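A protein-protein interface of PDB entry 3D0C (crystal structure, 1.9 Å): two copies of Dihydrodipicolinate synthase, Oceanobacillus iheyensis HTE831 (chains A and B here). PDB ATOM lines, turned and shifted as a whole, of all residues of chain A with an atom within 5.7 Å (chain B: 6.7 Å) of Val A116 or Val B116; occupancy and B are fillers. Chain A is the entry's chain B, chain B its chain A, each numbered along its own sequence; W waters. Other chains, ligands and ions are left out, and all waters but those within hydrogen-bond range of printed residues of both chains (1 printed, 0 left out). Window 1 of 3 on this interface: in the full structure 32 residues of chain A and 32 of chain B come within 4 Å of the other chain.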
ATOM      1  N   TYR A  60     -30.975  26.703   0.777  1.00  0.00           N
ATOM      2  CA  TYR A  60     -29.588  26.294   0.921  1.00  0.00           C
ATOM      3  C   TYR A  60     -29.075  26.208   2.357  1.00  0.00           C
ATOM      4  O   TYR A  60     -27.990  25.672   2.587  1.00  0.00           O
ATOM      5  CB  TYR A  60     -28.688  27.203   0.069  1.00  0.00           C
ATOM      6  CG  TYR A  60     -28.852  26.950  -1.418  1.00  0.00           C
ATOM      7  CD1 TYR A  60     -28.574  25.694  -1.965  1.00  0.00           C
ATOM      8  CD2 TYR A  60     -29.321  27.948  -2.273  1.00  0.00           C
ATOM      9  CE1 TYR A  60     -28.764  25.436  -3.321  1.00  0.00           C
ATOM     10  CE2 TYR A  60     -29.514  27.698  -3.636  1.00  0.00           C
ATOM     11  CZ  TYR A  60     -29.236  26.442  -4.151  1.00  0.00           C
ATOM     12  OH  TYR A  60     -29.444  26.184  -5.486  1.00  0.00           O
ATOM     13  N   TYR A  90     -28.892  21.313  -6.708  1.00  0.00           N
ATOM     14  CA  TYR A  90     -27.688  20.513  -6.465  1.00  0.00           C
ATOM     15  C   TYR A  90     -27.356  19.633  -7.671  1.00  0.00           C
ATOM     16  O   TYR A  90     -27.739  19.956  -8.793  1.00  0.00           O
ATOM     17  CB  TYR A  90     -27.852  19.658  -5.205  1.00  0.00           C
ATOM     18  CG  TYR A  90     -28.114  20.472  -3.958  1.00  0.00           C
ATOM     19  CD1 TYR A  90     -27.245  21.494  -3.570  1.00  0.00           C
ATOM     20  CD2 TYR A  90     -29.237  20.226  -3.166  1.00  0.00           C
ATOM     21  CE1 TYR A  90     -27.489  22.255  -2.419  1.00  0.00           C
ATOM     22  CE2 TYR A  90     -29.491  20.975  -2.018  1.00  0.00           C
ATOM     23  CZ  TYR A  90     -28.617  21.987  -1.648  1.00  0.00           C
ATOM     24  OH  TYR A  90     -28.878  22.723  -0.512  1.00  0.00           O
ATOM     25  N   GLN A 114     -31.114  27.835  -9.725  1.00  0.00           N
ATOM     26  CA  GLN A 114     -29.945  28.085 -10.557  1.00  0.00           C
ATOM     27  C   GLN A 114     -28.910  27.072 -10.084  1.00  0.00           C
ATOM     28  O   GLN A 114     -28.729  26.883  -8.882  1.00  0.00           O
ATOM     29  CB  GLN A 114     -29.384  29.494 -10.333  1.00  0.00           C
ATOM     30  CG  GLN A 114     -27.955  29.659 -10.884  1.00  0.00           C
ATOM     31  CD  GLN A 114     -27.378  31.061 -10.689  1.00  0.00           C
ATOM     32  OE1 GLN A 114     -27.634  31.724  -9.680  1.00  0.00           O
ATOM     33  NE2 GLN A 114     -26.574  31.506 -11.652  1.00  0.00           N
ATOM     34  N   PRO A 115     -28.234  26.384 -11.012  1.00  0.00           N
ATOM     35  CA  PRO A 115     -27.237  25.418 -10.540  1.00  0.00           C
ATOM     36  C   PRO A 115     -26.190  26.125  -9.662  1.00  0.00           C
ATOM     37  O   PRO A 115     -25.778  27.241  -9.972  1.00  0.00           O
ATOM     38  CB  PRO A 115     -26.630  24.888 -11.837  1.00  0.00           C
ATOM     39  CG  PRO A 115     -27.774  25.007 -12.825  1.00  0.00           C
ATOM     40  CD  PRO A 115     -28.395  26.335 -12.477  1.00  0.00           C
ATOM     41  N   VAL A 116     -25.767  25.484  -8.573  1.00  0.00           N
ATOM     42  CA  VAL A 116     -24.772  26.086  -7.680  1.00  0.00           C
ATOM     43  C   VAL A 116     -23.367  25.916  -8.238  1.00  0.00           C
ATOM     44  O   VAL A 116     -22.411  26.550  -7.772  1.00  0.00           O
ATOM     45  CB  VAL A 116     -24.801  25.454  -6.253  1.00  0.00           C
ATOM     46  CG1 VAL A 116     -26.134  25.744  -5.575  1.00  0.00           C
ATOM     47  CG2 VAL A 116     -24.556  23.951  -6.332  1.00  0.00           C
ATOM     48  N   HIS A 117     -23.254  25.054  -9.243  1.00  0.00           N
ATOM     49  CA  HIS A 117     -21.972  24.762  -9.874  1.00  0.00           C
ATOM     50  C   HIS A 117     -21.293  26.034 -10.357  1.00  0.00           C
ATOM     51  O   HIS A 117     -21.903  26.834 -11.058  1.00  0.00           O
ATOM     52  CB  HIS A 117     -22.184  23.819 -11.068  1.00  0.00           C
ATOM     53  CG  HIS A 117     -23.062  22.648 -10.764  1.00  0.00           C
ATOM     54  ND1 HIS A 117     -22.597  21.349 -10.753  1.00  0.00           N
ATOM     55  CD2 HIS A 117     -24.375  22.581 -10.436  1.00  0.00           C
ATOM     56  CE1 HIS A 117     -23.586  20.534 -10.432  1.00  0.00           C
ATOM     57  NE2 HIS A 117     -24.674  21.255 -10.233  1.00  0.00           N
ATOM     58  N   PRO A 118     -20.018  26.239  -9.989  1.00  0.00           N
ATOM     59  CA  PRO A 118     -19.306  27.443 -10.427  1.00  0.00           C
ATOM     60  C   PRO A 118     -18.994  27.445 -11.932  1.00  0.00           C
ATOM     61  O   PRO A 118     -18.774  28.503 -12.531  1.00  0.00           O
ATOM     62  CB  PRO A 118     -18.039  27.425  -9.569  1.00  0.00           C
ATOM     63  CG  PRO A 118     -17.798  25.970  -9.361  1.00  0.00           C
ATOM     64  CD  PRO A 118     -19.194  25.455  -9.053  1.00  0.00           C
ATOM     65  N   ASN B  55     -13.298  22.403  -6.675  1.00  0.00           N
ATOM     66  CA  ASN B  55     -14.149  22.592  -7.841  1.00  0.00           C
ATOM     67  C   ASN B  55     -13.535  21.934  -9.073  1.00  0.00           C
ATOM     68  O   ASN B  55     -14.244  21.612 -10.019  1.00  0.00           O
ATOM     69  CB  ASN B  55     -14.394  24.084  -8.084  1.00  0.00           C
ATOM     70  CG  ASN B  55     -15.436  24.661  -7.137  1.00  0.00           C
ATOM     71  OD1 ASN B  55     -15.314  25.794  -6.675  1.00  0.00           O
ATOM     72  ND2 ASN B  55     -16.475  23.883  -6.853  1.00  0.00           N
ATOM     73  N   TYR B  60     -19.538  19.966  -6.829  1.00  0.00           N
ATOM     74  CA  TYR B  60     -20.976  20.198  -6.897  1.00  0.00           C
ATOM     75  C   TYR B  60     -21.773  19.284  -7.835  1.00  0.00           C
ATOM     76  O   TYR B  60     -22.999  19.303  -7.814  1.00  0.00           O
ATOM     77  CB  TYR B  60     -21.249  21.674  -7.215  1.00  0.00           C
ATOM     78  CG  TYR B  60     -20.911  22.581  -6.050  1.00  0.00           C
ATOM     79  CD1 TYR B  60     -21.606  22.484  -4.841  1.00  0.00           C
ATOM     80  CD2 TYR B  60     -19.875  23.514  -6.140  1.00  0.00           C
ATOM     81  CE1 TYR B  60     -21.277  23.292  -3.751  1.00  0.00           C
ATOM     82  CE2 TYR B  60     -19.539  24.326  -5.054  1.00  0.00           C
ATOM     83  CZ  TYR B  60     -20.241  24.210  -3.865  1.00  0.00           C
ATOM     84  OH  TYR B  60     -19.914  25.010  -2.797  1.00  0.00           O
ATOM     85  N   GLY B  89     -18.872  21.899   1.969  1.00  0.00           N
ATOM     86  CA  GLY B  89     -19.737  23.026   1.686  1.00  0.00           C
ATOM     87  C   GLY B  89     -21.180  22.763   2.087  1.00  0.00           C
ATOM     88  O   GLY B  89     -21.462  21.881   2.903  1.00  0.00           O
ATOM     89  N   TYR B  90     -22.082  23.556   1.518  1.00  0.00           N
ATOM     90  CA  TYR B  90     -23.513  23.463   1.761  1.00  0.00           C
ATOM     91  C   TYR B  90     -23.903  24.063   3.113  1.00  0.00           C
ATOM     92  O   TYR B  90     -23.190  24.926   3.642  1.00  0.00           O
ATOM     93  CB  TYR B  90     -23.965  21.999   1.641  1.00  0.00           C
ATOM     94  CG  TYR B  90     -23.657  21.375   0.284  1.00  0.00           C
ATOM     95  CD1 TYR B  90     -24.164  21.932  -0.892  1.00  0.00           C
ATOM     96  CD2 TYR B  90     -22.875  20.216   0.176  1.00  0.00           C
ATOM     97  CE1 TYR B  90     -23.907  21.350  -2.149  1.00  0.00           C
ATOM     98  CE2 TYR B  90     -22.613  19.626  -1.075  1.00  0.00           C
ATOM     99  CZ  TYR B  90     -23.133  20.195  -2.229  1.00  0.00           C
ATOM    100  OH  TYR B  90     -22.895  19.600  -3.453  1.00  0.00           O
ATOM    101  N   SER B  91     -25.035  23.627   3.660  1.00  0.00           N
ATOM    102  CA  SER B  91     -25.518  24.146   4.947  1.00  0.00           C
ATOM    103  C   SER B  91     -24.527  23.818   6.072  1.00  0.00           C
ATOM    104  O   SER B  91     -23.729  22.894   5.948  1.00  0.00           O
ATOM    105  CB  SER B  91     -26.882  23.542   5.276  1.00  0.00           C
ATOM    106  OG  SER B  91     -26.748  22.206   5.747  1.00  0.00           O
ATOM    107  N   HIS B 113     -15.661  25.694   0.995  1.00  0.00           N
ATOM    108  CA  HIS B 113     -16.009  26.319  -0.269  1.00  0.00           C
ATOM    109  C   HIS B 113     -16.785  27.601  -0.012  1.00  0.00           C
ATOM    110  O   HIS B 113     -17.284  27.847   1.101  1.00  0.00           O
ATOM    111  CB  HIS B 113     -16.921  25.385  -1.081  1.00  0.00           C
ATOM    112  CG  HIS B 113     -16.198  24.330  -1.859  1.00  0.00           C
ATOM    113  ND1 HIS B 113     -15.649  24.569  -3.102  1.00  0.00           N
ATOM    114  CD2 HIS B 113     -15.987  23.015  -1.607  1.00  0.00           C
ATOM    115  CE1 HIS B 113     -15.140  23.452  -3.581  1.00  0.00           C
ATOM    116  NE2 HIS B 113     -15.330  22.490  -2.693  1.00  0.00           N
ATOM    117  N   GLN B 114     -16.893  28.416  -1.052  1.00  0.00           N
ATOM    118  CA  GLN B 114     -17.674  29.636  -0.955  1.00  0.00           C
ATOM    119  C   GLN B 114     -19.102  29.158  -0.720  1.00  0.00           C
ATOM    120  O   GLN B 114     -19.589  28.235  -1.395  1.00  0.00           O
ATOM    121  CB  GLN B 114     -17.617  30.440  -2.261  1.00  0.00           C
ATOM    122  CG  GLN B 114     -18.734  31.474  -2.391  1.00  0.00           C
ATOM    123  CD  GLN B 114     -18.711  32.227  -3.712  1.00  0.00           C
ATOM    124  OE1 GLN B 114     -18.446  31.652  -4.774  1.00  0.00           O
ATOM    125  NE2 GLN B 114     -19.012  33.520  -3.655  1.00  0.00           N
ATOM    126  N   PRO B 115     -19.789  29.758   0.255  1.00  0.00           N
ATOM    127  CA  PRO B 115     -21.171  29.354   0.534  1.00  0.00           C
ATOM    128  C   PRO B 115     -22.038  29.476  -0.721  1.00  0.00           C
ATOM    129  O   PRO B 115     -22.000  30.499  -1.403  1.00  0.00           O
ATOM    130  CB  PRO B 115     -21.601  30.335   1.619  1.00  0.00           C
ATOM    131  CG  PRO B 115     -20.308  30.642   2.340  1.00  0.00           C
ATOM    132  CD  PRO B 115     -19.306  30.763   1.221  1.00  0.00           C
ATOM    133  N   VAL B 116     -22.813  28.441  -1.033  1.00  0.00           N
ATOM    134  CA  VAL B 116     -23.679  28.488  -2.210  1.00  0.00           C
ATOM    135  C   VAL B 116     -24.882  29.401  -1.983  1.00  0.00           C
ATOM    136  O   VAL B 116     -25.560  29.789  -2.932  1.00  0.00           O
ATOM    137  CB  VAL B 116     -24.207  27.078  -2.605  1.00  0.00           C
ATOM    138  CG1 VAL B 116     -23.035  26.158  -2.966  1.00  0.00           C
ATOM    139  CG2 VAL B 116     -25.021  26.481  -1.465  1.00  0.00           C
ATOM    140  N   HIS B 117     -25.148  29.754  -0.730  1.00  0.00           N
ATOM    141  CA  HIS B 117     -26.297  30.614  -0.437  1.00  0.00           C
ATOM    142  C   HIS B 117     -26.251  31.913  -1.239  1.00  0.00           C
ATOM    143  O   HIS B 117     -25.211  32.563  -1.293  1.00  0.00           O
ATOM    144  CB  HIS B 117     -26.343  30.975   1.050  1.00  0.00           C
ATOM    145  CG  HIS B 117     -26.195  29.805   1.970  1.00  0.00           C
ATOM    146  ND1 HIS B 117     -25.043  29.053   2.032  1.00  0.00           N
ATOM    147  CD2 HIS B 117     -27.033  29.292   2.900  1.00  0.00           C
ATOM    148  CE1 HIS B 117     -25.175  28.129   2.969  1.00  0.00           C
ATOM    149  NE2 HIS B 117     -26.373  28.254   3.511  1.00  0.00           N
ATOM    150  N   PRO B 118     -27.378  32.309  -1.869  1.00  0.00           N
ATOM    151  CA  PRO B 118     -27.426  33.549  -2.654  1.00  0.00           C
ATOM    152  C   PRO B 118     -27.412  34.798  -1.768  1.00  0.00           C
ATOM    153  O   PRO B 118     -27.086  35.893  -2.233  1.00  0.00           O
ATOM    154  CB  PRO B 118     -28.734  33.420  -3.443  1.00  0.00           C
ATOM    155  CG  PRO B 118     -29.590  32.591  -2.544  1.00  0.00           C
ATOM    156  CD  PRO B 118     -28.614  31.530  -2.062  1.00  0.00           C
ATOM    157  N   TYR B 119     -27.760  34.620  -0.491  1.00  0.00           N
ATOM    158  CA  TYR B 119     -27.789  35.726   0.469  1.00  0.00           C
ATOM    159  C   TYR B 119     -26.806  35.472   1.608  1.00  0.00           C
ATOM    160  O   TYR B 119     -26.885  34.456   2.306  1.00  0.00           O
ATOM    161  CB  TYR B 119     -29.201  35.906   1.044  1.00  0.00           C
ATOM    162  CG  TYR B 119     -30.313  35.797   0.021  1.00  0.00           C
ATOM    163  CD1 TYR B 119     -30.234  36.461  -1.203  1.00  0.00           C
ATOM    164  CD2 TYR B 119     -31.449  35.028   0.280  1.00  0.00           C
ATOM    165  CE1 TYR B 119     -31.258  36.359  -2.148  1.00  0.00           C
ATOM    166  CE2 TYR B 119     -32.478  34.922  -0.657  1.00  0.00           C
ATOM    167  CZ  TYR B 119     -32.374  35.590  -1.869  1.00  0.00           C
ATOM    168  OH  TYR B 119     -33.378  35.477  -2.802  1.00  0.00           O
ATOM    169  N   TYR B 128     -21.146  31.450  10.110  1.00  0.00           N
ATOM    170  CA  TYR B 128     -21.129  30.262   9.260  1.00  0.00           C
ATOM    171  C   TYR B 128     -19.777  29.572   9.392  1.00  0.00           C
ATOM    172  O   TYR B 128     -19.682  28.385   9.755  1.00  0.00           O
ATOM    173  CB  TYR B 128     -21.351  30.678   7.799  1.00  0.00           C
ATOM    174  CG  TYR B 128     -21.299  29.540   6.812  1.00  0.00           C
ATOM    175  CD1 TYR B 128     -22.398  28.707   6.623  1.00  0.00           C
ATOM    176  CD2 TYR B 128     -20.145  29.287   6.071  1.00  0.00           C
ATOM    177  CE1 TYR B 128     -22.351  27.647   5.719  1.00  0.00           C
ATOM    178  CE2 TYR B 128     -20.084  28.236   5.169  1.00  0.00           C
ATOM    179  CZ  TYR B 128     -21.190  27.417   4.995  1.00  0.00           C
ATOM    180  OH  TYR B 128     -21.121  26.378   4.098  1.00  0.00           O
HETATM  181  O   HOH W   1     -26.740  23.999   0.893  1.00  0.00           O
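The backbone carbonyl oxygen (O) of Tyr A60 is in hydrogen-bond range of a ring nitrogen (NE2) of His B117, at 3.2 Å.
The backbone carbonyl oxygen of Tyr B90 is in hydrogen-bond range of the side-chain hydroxyl of Tyr B128, 2.6 Å away.
O of Tyr A60 touches CB of Ser B91 (3.6 Å).
Val B116 touches Tyr A60 (CG2 to CD1, 3.7 Å).
CD2 of Tyr A60 touches CD of Pro B118, at 3.7 Å.
CD1 of Tyr A90 touches CE1 of Tyr B90 (3.6 Å).
Val A116 touches Tyr B60.
Val B116 touches Val A116.
Tyr B60 touches His A117.
CG of Asn B55 touches CG of Pro A118 (3.5 Å).
Tyr B60 touches Pro A118 (CD2 to CD, 3.6 Å).
Printed residues of chain B within 4 Å of Tyr A60: Ser B91, Val B116, His B117 and Pro B118.
Pro A115 touches none of the printed residues of chain B.
Of chain B, only Tyr B60 (3.6 Å) and Val B116 (3.8 Å) come within 4 Å of Val A116.
Of the printed residues of chain A, Asn B55 touches Pro A118.
Of the printed residues of chain A, Tyr B60 touches Val A116, His A117 and Pro A118.
Gly B89 touches none of the printed residues of chain A.
Printed residues of chain A within 4 Å of Ser B91: Tyr A60.
Val B116 touches just these residues of chain A: Tyr A60 and Val A116.
The nearest printed residue of chain B that does not touch Pro A118 is Gln B114 (6.4 Å).
Of the 7 printed residues of chain A, 5 touch a printed residue of chain B.
Hydrophobic or aromatic side chains of chain A that line the printed part of chain B: Tyr A60, Tyr A90, Val A116, His A117 and Pro A118.
Along chain A the printed residues that touch a printed residue of chain B span positions 60 to 118.
Of the 13 printed residues of chain B, 7 touch a printed residue of chain A.
Along chain B the printed residues that touch a printed residue of chain A span positions 55 to 118.
Among the printed residues, no Asp or Glu carboxylate lies within 4 Å of a Lys or Arg side-chain nitrogen of the other chain.
Tyr A60 touches Val B116, and with the chains exchanged Val A116 touches Tyr B60.
Tyr A60 touches Pro B118, and with the chains exchanged Pro A118 touches Tyr B60.
Tyr B90 touches its own counterpart, Tyr A90.
Val A116 touches its own counterpart, Val B116.
Positions printed for both chains: 60, 90, 114, 115, 116, 117 and 118.
Of the 10 pairs that touch across the chains among the printed residues, 8 have their exchanged pair printed and touching as well.
Water W1 lies within hydrogen-bond range of the backbone carbonyl oxygen (O) of Tyr A60, the side-chain hydroxyl (OH) of Tyr A90 and the backbone NH (N) of Ser B91.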
